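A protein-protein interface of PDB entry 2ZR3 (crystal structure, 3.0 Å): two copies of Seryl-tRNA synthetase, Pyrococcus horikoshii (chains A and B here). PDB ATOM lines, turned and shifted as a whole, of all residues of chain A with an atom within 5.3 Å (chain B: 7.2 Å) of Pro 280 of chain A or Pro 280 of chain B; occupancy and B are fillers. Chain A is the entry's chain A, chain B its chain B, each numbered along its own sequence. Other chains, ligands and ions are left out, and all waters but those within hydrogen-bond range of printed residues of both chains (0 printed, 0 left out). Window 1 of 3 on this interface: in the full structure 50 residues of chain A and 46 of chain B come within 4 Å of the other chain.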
ATOM      1  N   TYR A 219     -15.136  11.730  11.170  1.00  0.00           N
ATOM      2  CA  TYR A 219     -14.060  11.275  12.040  1.00  0.00           C
ATOM      3  C   TYR A 219     -14.053   9.751  12.184  1.00  0.00           C
ATOM      4  O   TYR A 219     -13.081   9.167  12.664  1.00  0.00           O
ATOM      5  CB  TYR A 219     -14.199  11.964  13.402  1.00  0.00           C
ATOM      6  CG  TYR A 219     -14.168  13.474  13.302  1.00  0.00           C
ATOM      7  CD1 TYR A 219     -14.682  14.276  14.315  1.00  0.00           C
ATOM      8  CD2 TYR A 219     -13.628  14.103  12.181  1.00  0.00           C
ATOM      9  CE1 TYR A 219     -14.656  15.681  14.207  1.00  0.00           C
ATOM     10  CE2 TYR A 219     -13.597  15.492  12.065  1.00  0.00           C
ATOM     11  CZ  TYR A 219     -14.113  16.278  13.076  1.00  0.00           C
ATOM     12  OH  TYR A 219     -14.102  17.648  12.935  1.00  0.00           O
ATOM     13  N   ILE A 250     -10.601   7.677  12.582  1.00  0.00           N
ATOM     14  CA  ILE A 250      -9.518   8.085  11.698  1.00  0.00           C
ATOM     15  C   ILE A 250      -8.272   8.563  12.422  1.00  0.00           C
ATOM     16  O   ILE A 250      -8.344   9.259  13.432  1.00  0.00           O
ATOM     17  CB  ILE A 250      -9.964   9.207  10.724  1.00  0.00           C
ATOM     18  CG1 ILE A 250     -10.358  10.455  11.505  1.00  0.00           C
ATOM     19  CG2 ILE A 250     -11.161   8.745   9.886  1.00  0.00           C
ATOM     20  CD1 ILE A 250     -10.377  11.689  10.660  1.00  0.00           C
ATOM     21  N   VAL A 278      -9.262  19.144   8.039  1.00  0.00           N
ATOM     22  CA  VAL A 278      -9.086  19.413   9.460  1.00  0.00           C
ATOM     23  C   VAL A 278      -9.856  18.354  10.202  1.00  0.00           C
ATOM     24  O   VAL A 278     -11.005  18.074   9.874  1.00  0.00           O
ATOM     25  CB  VAL A 278      -9.712  20.740   9.908  1.00  0.00           C
ATOM     26  CG1 VAL A 278      -8.860  21.364  11.002  1.00  0.00           C
ATOM     27  CG2 VAL A 278      -9.884  21.663   8.739  1.00  0.00           C
ATOM     28  N   SER A 279      -9.241  17.776  11.216  1.00  0.00           N
ATOM     29  CA  SER A 279      -9.936  16.772  11.974  1.00  0.00           C
ATOM     30  C   SER A 279      -9.140  16.348  13.177  1.00  0.00           C
ATOM     31  O   SER A 279      -7.925  16.549  13.237  1.00  0.00           O
ATOM     32  CB  SER A 279     -10.173  15.536  11.115  1.00  0.00           C
ATOM     33  OG  SER A 279      -8.976  14.790  10.987  1.00  0.00           O
ATOM     34  N   PRO A 280      -9.829  15.807  14.187  1.00  0.00           N
ATOM     35  CA  PRO A 280      -9.081  15.356  15.356  1.00  0.00           C
ATOM     36  C   PRO A 280      -8.461  14.062  14.832  1.00  0.00           C
ATOM     37  O   PRO A 280      -8.948  13.498  13.848  1.00  0.00           O
ATOM     38  CB  PRO A 280     -10.175  15.120  16.400  1.00  0.00           C
ATOM     39  CG  PRO A 280     -11.401  14.850  15.575  1.00  0.00           C
ATOM     40  CD  PRO A 280     -11.274  15.847  14.464  1.00  0.00           C
ATOM     41  N   CYS A 281      -7.376  13.606  15.443  1.00  0.00           N
ATOM     42  CA  CYS A 281      -6.735  12.381  14.985  1.00  0.00           C
ATOM     43  C   CYS A 281      -6.621  11.450  16.158  1.00  0.00           C
ATOM     44  O   CYS A 281      -6.226  11.888  17.233  1.00  0.00           O
ATOM     45  CB  CYS A 281      -5.340  12.673  14.431  1.00  0.00           C
ATOM     46  SG  CYS A 281      -5.317  13.670  12.927  1.00  0.00           S
ATOM     47  N   PHE A 282      -6.971  10.179  15.958  1.00  0.00           N
ATOM     48  CA  PHE A 282      -6.886   9.190  17.031  1.00  0.00           C
ATOM     49  C   PHE A 282      -5.907   8.093  16.649  1.00  0.00           C
ATOM     50  O   PHE A 282      -5.998   7.534  15.563  1.00  0.00           O
ATOM     51  CB  PHE A 282      -8.257   8.583  17.308  1.00  0.00           C
ATOM     52  CG  PHE A 282      -9.338   9.601  17.492  1.00  0.00           C
ATOM     53  CD1 PHE A 282     -10.026  10.111  16.395  1.00  0.00           C
ATOM     54  CD2 PHE A 282      -9.661  10.066  18.757  1.00  0.00           C
ATOM     55  CE1 PHE A 282     -11.030  11.076  16.558  1.00  0.00           C
ATOM     56  CE2 PHE A 282     -10.661  11.030  18.932  1.00  0.00           C
ATOM     57  CZ  PHE A 282     -11.345  11.534  17.825  1.00  0.00           C
ATOM     58  N   PHE A 302      -5.079  14.332  18.785  1.00  0.00           N
ATOM     59  CA  PHE A 302      -4.540  15.622  18.412  1.00  0.00           C
ATOM     60  C   PHE A 302      -5.213  16.142  17.173  1.00  0.00           C
ATOM     61  O   PHE A 302      -5.921  15.417  16.486  1.00  0.00           O
ATOM     62  CB  PHE A 302      -3.060  15.535  18.146  1.00  0.00           C
ATOM     63  CG  PHE A 302      -2.700  14.524  17.113  1.00  0.00           C
ATOM     64  CD1 PHE A 302      -2.563  13.184  17.458  1.00  0.00           C
ATOM     65  CD2 PHE A 302      -2.476  14.907  15.791  1.00  0.00           C
ATOM     66  CE1 PHE A 302      -2.204  12.240  16.501  1.00  0.00           C
ATOM     67  CE2 PHE A 302      -2.117  13.967  14.824  1.00  0.00           C
ATOM     68  CZ  PHE A 302      -1.980  12.633  15.180  1.00  0.00           C
ATOM     69  N   HIS A 303      -4.957  17.405  16.880  1.00  0.00           N
ATOM     70  CA  HIS A 303      -5.545  18.053  15.733  1.00  0.00           C
ATOM     71  C   HIS A 303      -4.506  18.222  14.634  1.00  0.00           C
ATOM     72  O   HIS A 303      -3.349  18.496  14.911  1.00  0.00           O
ATOM     73  CB  HIS A 303      -6.088  19.399  16.178  1.00  0.00           C
ATOM     74  CG  HIS A 303      -7.110  19.298  17.261  1.00  0.00           C
ATOM     75  ND1 HIS A 303      -7.489  20.375  18.033  1.00  0.00           N
ATOM     76  CD2 HIS A 303      -7.871  18.254  17.674  1.00  0.00           C
ATOM     77  CE1 HIS A 303      -8.442  20.001  18.871  1.00  0.00           C
ATOM     78  NE2 HIS A 303      -8.693  18.718  18.673  1.00  0.00           N
ATOM     79  N   ILE B 216      -9.747  22.088  26.235  1.00  0.00           N
ATOM     80  CA  ILE B 216      -9.892  21.079  25.203  1.00  0.00           C
ATOM     81  C   ILE B 216      -9.698  19.836  26.045  1.00  0.00           C
ATOM     82  O   ILE B 216      -8.665  19.666  26.683  1.00  0.00           O
ATOM     83  CB  ILE B 216      -8.792  21.181  24.129  1.00  0.00           C
ATOM     84  CG1 ILE B 216      -8.961  22.490  23.345  1.00  0.00           C
ATOM     85  CG2 ILE B 216      -8.872  19.980  23.187  1.00  0.00           C
ATOM     86  CD1 ILE B 216      -7.968  22.685  22.223  1.00  0.00           C
ATOM     87  N   PRO B 217     -10.702  18.962  26.088  1.00  0.00           N
ATOM     88  CA  PRO B 217     -10.560  17.761  26.905  1.00  0.00           C
ATOM     89  C   PRO B 217     -10.276  16.515  26.115  1.00  0.00           C
ATOM     90  O   PRO B 217     -10.147  16.555  24.892  1.00  0.00           O
ATOM     91  CB  PRO B 217     -11.916  17.671  27.568  1.00  0.00           C
ATOM     92  CG  PRO B 217     -12.804  17.985  26.402  1.00  0.00           C
ATOM     93  CD  PRO B 217     -12.112  19.157  25.709  1.00  0.00           C
ATOM     94  N   PRO B 218     -10.150  15.385  26.817  1.00  0.00           N
ATOM     95  CA  PRO B 218      -9.893  14.114  26.135  1.00  0.00           C
ATOM     96  C   PRO B 218     -11.208  13.792  25.444  1.00  0.00           C
ATOM     97  O   PRO B 218     -12.274  14.080  25.987  1.00  0.00           O
ATOM     98  CB  PRO B 218      -9.591  13.167  27.285  1.00  0.00           C
ATOM     99  CG  PRO B 218      -8.917  14.080  28.275  1.00  0.00           C
ATOM    100  CD  PRO B 218      -9.819  15.292  28.246  1.00  0.00           C
ATOM    101  N   TYR B 219     -11.146  13.231  24.250  1.00  0.00           N
ATOM    102  CA  TYR B 219     -12.370  12.924  23.524  1.00  0.00           C
ATOM    103  C   TYR B 219     -12.842  11.519  23.828  1.00  0.00           C
ATOM    104  O   TYR B 219     -13.933  11.123  23.427  1.00  0.00           O
ATOM    105  CB  TYR B 219     -12.152  13.089  22.020  1.00  0.00           C
ATOM    106  CG  TYR B 219     -11.679  14.471  21.617  1.00  0.00           C
ATOM    107  CD1 TYR B 219     -11.161  14.696  20.346  1.00  0.00           C
ATOM    108  CD2 TYR B 219     -11.781  15.562  22.492  1.00  0.00           C
ATOM    109  CE1 TYR B 219     -10.757  15.976  19.943  1.00  0.00           C
ATOM    110  CE2 TYR B 219     -11.382  16.851  22.094  1.00  0.00           C
ATOM    111  CZ  TYR B 219     -10.874  17.044  20.811  1.00  0.00           C
ATOM    112  OH  TYR B 219     -10.513  18.295  20.365  1.00  0.00           O
ATOM    113  N   LEU B 249     -16.307   7.098  23.394  1.00  0.00           N
ATOM    114  CA  LEU B 249     -16.300   8.364  22.676  1.00  0.00           C
ATOM    115  C   LEU B 249     -17.291   9.318  23.340  1.00  0.00           C
ATOM    116  O   LEU B 249     -18.454   8.977  23.521  1.00  0.00           O
ATOM    117  CB  LEU B 249     -16.680   8.156  21.210  1.00  0.00           C
ATOM    118  CG  LEU B 249     -15.728   7.366  20.315  1.00  0.00           C
ATOM    119  CD1 LEU B 249     -16.120   7.583  18.856  1.00  0.00           C
ATOM    120  CD2 LEU B 249     -14.319   7.852  20.511  1.00  0.00           C
ATOM    121  N   ILE B 250     -16.832  10.520  23.671  1.00  0.00           N
ATOM    122  CA  ILE B 250     -17.669  11.499  24.344  1.00  0.00           C
ATOM    123  C   ILE B 250     -18.751  12.154  23.477  1.00  0.00           C
ATOM    124  O   ILE B 250     -18.520  12.553  22.342  1.00  0.00           O
ATOM    125  CB  ILE B 250     -16.803  12.636  24.993  1.00  0.00           C
ATOM    126  CG1 ILE B 250     -16.253  13.567  23.920  1.00  0.00           C
ATOM    127  CG2 ILE B 250     -15.621  12.051  25.752  1.00  0.00           C
ATOM    128  CD1 ILE B 250     -15.917  14.895  24.459  1.00  0.00           C
ATOM    129  N   PRO B 251     -19.962  12.267  24.015  1.00  0.00           N
ATOM    130  CA  PRO B 251     -21.052  12.883  23.263  1.00  0.00           C
ATOM    131  C   PRO B 251     -21.170  14.364  23.568  1.00  0.00           C
ATOM    132  O   PRO B 251     -22.090  15.027  23.092  1.00  0.00           O
ATOM    133  CB  PRO B 251     -22.261  12.136  23.772  1.00  0.00           C
ATOM    134  CG  PRO B 251     -21.911  11.968  25.226  1.00  0.00           C
ATOM    135  CD  PRO B 251     -20.480  11.538  25.189  1.00  0.00           C
ATOM    136  N   THR B 252     -20.239  14.885  24.359  1.00  0.00           N
ATOM    137  CA  THR B 252     -20.299  16.284  24.760  1.00  0.00           C
ATOM    138  C   THR B 252     -19.140  16.619  25.671  1.00  0.00           C
ATOM    139  O   THR B 252     -18.800  15.845  26.543  1.00  0.00           O
ATOM    140  CB  THR B 252     -21.594  16.554  25.541  1.00  0.00           C
ATOM    141  OG1 THR B 252     -21.517  17.824  26.208  1.00  0.00           O
ATOM    142  CG2 THR B 252     -21.816  15.443  26.574  1.00  0.00           C
ATOM    143  N   ALA B 253     -18.539  17.786  25.482  1.00  0.00           N
ATOM    144  CA  ALA B 253     -17.427  18.192  26.327  1.00  0.00           C
ATOM    145  C   ALA B 253     -17.841  18.197  27.790  1.00  0.00           C
ATOM    146  O   ALA B 253     -17.015  18.424  28.670  1.00  0.00           O
ATOM    147  CB  ALA B 253     -16.971  19.557  25.933  1.00  0.00           C
ATOM    148  N   VAL B 278     -14.438  22.654  24.371  1.00  0.00           N
ATOM    149  CA  VAL B 278     -14.672  22.554  22.930  1.00  0.00           C
ATOM    150  C   VAL B 278     -14.313  21.133  22.597  1.00  0.00           C
ATOM    151  O   VAL B 278     -13.348  20.605  23.141  1.00  0.00           O
ATOM    152  CB  VAL B 278     -13.719  23.412  22.082  1.00  0.00           C
ATOM    153  CG1 VAL B 278     -14.255  23.486  20.665  1.00  0.00           C
ATOM    154  CG2 VAL B 278     -13.546  24.778  22.682  1.00  0.00           C
ATOM    155  N   SER B 279     -15.063  20.500  21.712  1.00  0.00           N
ATOM    156  CA  SER B 279     -14.723  19.129  21.350  1.00  0.00           C
ATOM    157  C   SER B 279     -15.653  18.568  20.319  1.00  0.00           C
ATOM    158  O   SER B 279     -16.719  19.111  20.059  1.00  0.00           O
ATOM    159  CB  SER B 279     -14.796  18.198  22.564  1.00  0.00           C
ATOM    160  OG  SER B 279     -16.128  17.738  22.756  1.00  0.00           O
ATOM    161  N   PRO B 280     -15.232  17.483  19.680  1.00  0.00           N
ATOM    162  CA  PRO B 280     -16.104  16.863  18.686  1.00  0.00           C
ATOM    163  C   PRO B 280     -17.057  16.096  19.592  1.00  0.00           C
ATOM    164  O   PRO B 280     -16.752  15.876  20.770  1.00  0.00           O
ATOM    165  CB  PRO B 280     -15.166  15.924  17.939  1.00  0.00           C
ATOM    166  CG  PRO B 280     -13.837  16.604  18.059  1.00  0.00           C
ATOM    167  CD  PRO B 280     -13.834  17.071  19.490  1.00  0.00           C
ATOM    168  N   CYS B 281     -18.206  15.712  19.066  1.00  0.00           N
ATOM    169  CA  CYS B 281     -19.181  14.979  19.852  1.00  0.00           C
ATOM    170  C   CYS B 281     -19.649  13.825  19.037  1.00  0.00           C
ATOM    171  O   CYS B 281     -19.887  13.979  17.846  1.00  0.00           O
ATOM    172  CB  CYS B 281     -20.358  15.869  20.192  1.00  0.00           C
ATOM    173  SG  CYS B 281     -19.871  17.146  21.308  1.00  0.00           S
ATOM    174  N   PHE B 282     -19.782  12.667  19.665  1.00  0.00           N
ATOM    175  CA  PHE B 282     -20.232  11.503  18.930  1.00  0.00           C
ATOM    176  C   PHE B 282     -21.457  10.928  19.572  1.00  0.00           C
ATOM    177  O   PHE B 282     -21.497  10.722  20.784  1.00  0.00           O
ATOM    178  CB  PHE B 282     -19.127  10.463  18.860  1.00  0.00           C
ATOM    179  CG  PHE B 282     -17.846  11.002  18.318  1.00  0.00           C
ATOM    180  CD1 PHE B 282     -16.971  11.704  19.142  1.00  0.00           C
ATOM    181  CD2 PHE B 282     -17.535  10.858  16.969  1.00  0.00           C
ATOM    182  CE1 PHE B 282     -15.807  12.257  18.637  1.00  0.00           C
ATOM    183  CE2 PHE B 282     -16.374  11.407  16.452  1.00  0.00           C
ATOM    184  CZ  PHE B 282     -15.502  12.113  17.294  1.00  0.00           C
ATOM    185  N   GLN B 301     -21.699  12.959  14.398  1.00  0.00           N
ATOM    186  CA  GLN B 301     -20.610  13.784  14.897  1.00  0.00           C
ATOM    187  C   GLN B 301     -20.871  15.242  14.628  1.00  0.00           C
ATOM    188  O   GLN B 301     -21.469  15.613  13.621  1.00  0.00           O
ATOM    189  CB  GLN B 301     -19.262  13.370  14.276  1.00  0.00           C
ATOM    190  CG  GLN B 301     -18.776  14.223  13.113  1.00  0.00           C
ATOM    191  CD  GLN B 301     -17.646  13.562  12.334  1.00  0.00           C
ATOM    192  OE1 GLN B 301     -17.759  12.411  11.944  1.00  0.00           O
ATOM    193  NE2 GLN B 301     -16.570  14.294  12.084  1.00  0.00           N
ATOM    194  N   PHE B 302     -20.429  16.072  15.555  1.00  0.00           N
ATOM    195  CA  PHE B 302     -20.583  17.497  15.408  1.00  0.00           C
ATOM    196  C   PHE B 302     -19.685  18.142  16.425  1.00  0.00           C
ATOM    197  O   PHE B 302     -19.176  17.478  17.320  1.00  0.00           O
ATOM    198  CB  PHE B 302     -22.029  17.931  15.636  1.00  0.00           C
ATOM    199  CG  PHE B 302     -22.554  17.607  17.000  1.00  0.00           C
ATOM    200  CD1 PHE B 302     -22.976  16.325  17.309  1.00  0.00           C
ATOM    201  CD2 PHE B 302     -22.650  18.594  17.975  1.00  0.00           C
ATOM    202  CE1 PHE B 302     -23.495  16.029  18.571  1.00  0.00           C
ATOM    203  CE2 PHE B 302     -23.167  18.305  19.243  1.00  0.00           C
ATOM    204  CZ  PHE B 302     -23.589  17.016  19.535  1.00  0.00           C
ATOM    205  N   HIS B 303     -19.489  19.441  16.269  1.00  0.00           N
ATOM    206  CA  HIS B 303     -18.641  20.189  17.172  1.00  0.00           C
ATOM    207  C   HIS B 303     -19.547  20.974  18.096  1.00  0.00           C
ATOM    208  O   HIS B 303     -20.632  21.394  17.697  1.00  0.00           O
ATOM    209  CB  HIS B 303     -17.752  21.149  16.373  1.00  0.00           C
ATOM    210  CG  HIS B 303     -16.775  20.459  15.479  1.00  0.00           C
ATOM    211  ND1 HIS B 303     -16.202  21.074  14.387  1.00  0.00           N
ATOM    212  CD2 HIS B 303     -16.261  19.207  15.518  1.00  0.00           C
ATOM    213  CE1 HIS B 303     -15.379  20.230  13.789  1.00  0.00           C
ATOM    214  NE2 HIS B 303     -15.398  19.088  14.455  1.00  0.00           N
ATOM    215  N   LYS B 304     -19.107  21.178  19.328  1.00  0.00           N
ATOM    216  CA  LYS B 304     -19.908  21.933  20.276  1.00  0.00           C
ATOM    217  C   LYS B 304     -19.077  22.562  21.386  1.00  0.00           C
ATOM    218  O   LYS B 304     -18.181  21.919  21.945  1.00  0.00           O
ATOM    219  CB  LYS B 304     -20.990  21.028  20.890  1.00  0.00           C
ATOM    220  CG  LYS B 304     -21.670  21.655  22.086  1.00  0.00           C
ATOM    221  CD  LYS B 304     -22.953  20.960  22.470  1.00  0.00           C
ATOM    222  CE  LYS B 304     -22.743  19.660  23.199  1.00  0.00           C
ATOM    223  NZ  LYS B 304     -24.017  19.381  23.911  1.00  0.00           N
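Among the printed residues, pairs that only touch across the chains: Tyr 219 of chain A with Pro 280 of chain B (3.8 Å), Tyr 219 of chain A with Phe 282 of chain B (3.8 Å), Pro 280 of chain A with Tyr 219 of chain B (3.7 Å), Pro 280 of chain A with Pro 280 of chain B (3.9 Å) and Phe 282 of chain A with Tyr 219 of chain B (3.96 Å).
Tyr 219 of chain A touches Pro 280 of chain B, and with the chains exchanged Pro 280 of chain A touches Tyr 219 of chain B.
Tyr 219 of chain A touches Phe 282 of chain B, and with the chains exchanged Phe 282 of chain A touches Tyr 219 of chain B.
Tyr 219 of chain A touches His 303 of chain B, and with the chains exchanged His 303 of chain A touches Tyr 219 of chain B.
Pro 280 of chain A touches its own counterpart, Pro 280 of chain B.
Of the 8 pairs that touch across the chains among the printed residues, 7 have their exchanged pair printed and touching as well.
Of the 18 printed residues of chain B, 5 touch a printed residue of chain A.
Among the printed residues, 8 pairs touch across the chains.
Among the printed residues, no Asp or Glu carboxylate lies within 4 Å of a Lys or Arg side-chain nitrogen of the other chain.
N of Ile 250 of chain B lies within hydrogen-bond range of O of Tyr 219 of chain B.
The backbone carbonyl oxygen of Ile 250 of chain B lies within hydrogen-bond range of the backbone NH of Phe 282 of chain B (3.0 Å).
The backbone carbonyl oxygen (O) of Ile 250 of chain A is in hydrogen-bond range of the backbone NH (N) of Phe 282 of chain A (3.0 Å).
N of Ile 250 of chain A is in hydrogen-bond range of O of Tyr 219 of chain A.
The side-chain amide oxygen of Gln 301 of chain B sits at hydrogen-bond distance from the backbone NH of Tyr 219 of chain A (2.8 Å).
A ring nitrogen (NE2) of His 303 of chain A is in hydrogen-bond range of the side-chain hydroxyl (OH) of Tyr 219 of chain B, at 2.5 Å.
The side-chain hydroxyl of Tyr 219 of chain A sits at hydrogen-bond distance from a ring nitrogen (NE2) of His 303 of chain B (2.5 Å).
Of the printed residues of chain B, Tyr 219 of chain A touches Pro 280, Phe 282, Gln 301 and His 303.
Pro 280 of chain A touches just these residues of chain B: Tyr 219 and Pro 280.
Pro 218 of chain B touches none of the printed residues of chain A.
Of the printed residues of chain A, Tyr 219 of chain B touches Pro 280 (3.7 Å), Phe 282 (3.96 Å) and His 303 (2.5 Å).
Pro 280 of chain B touches two residues of chain A.
Printed residues of chain A within 4 Å of Phe 282 of chain B: Tyr 219.
The nearest printed residue of chain A that does not touch Pro 280 of chain B is His 303 of chain A (5.5 Å).
The nearest printed residue of chain A that does not touch Gln 301 of chain B is Pro 280 of chain A (6.0 Å).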
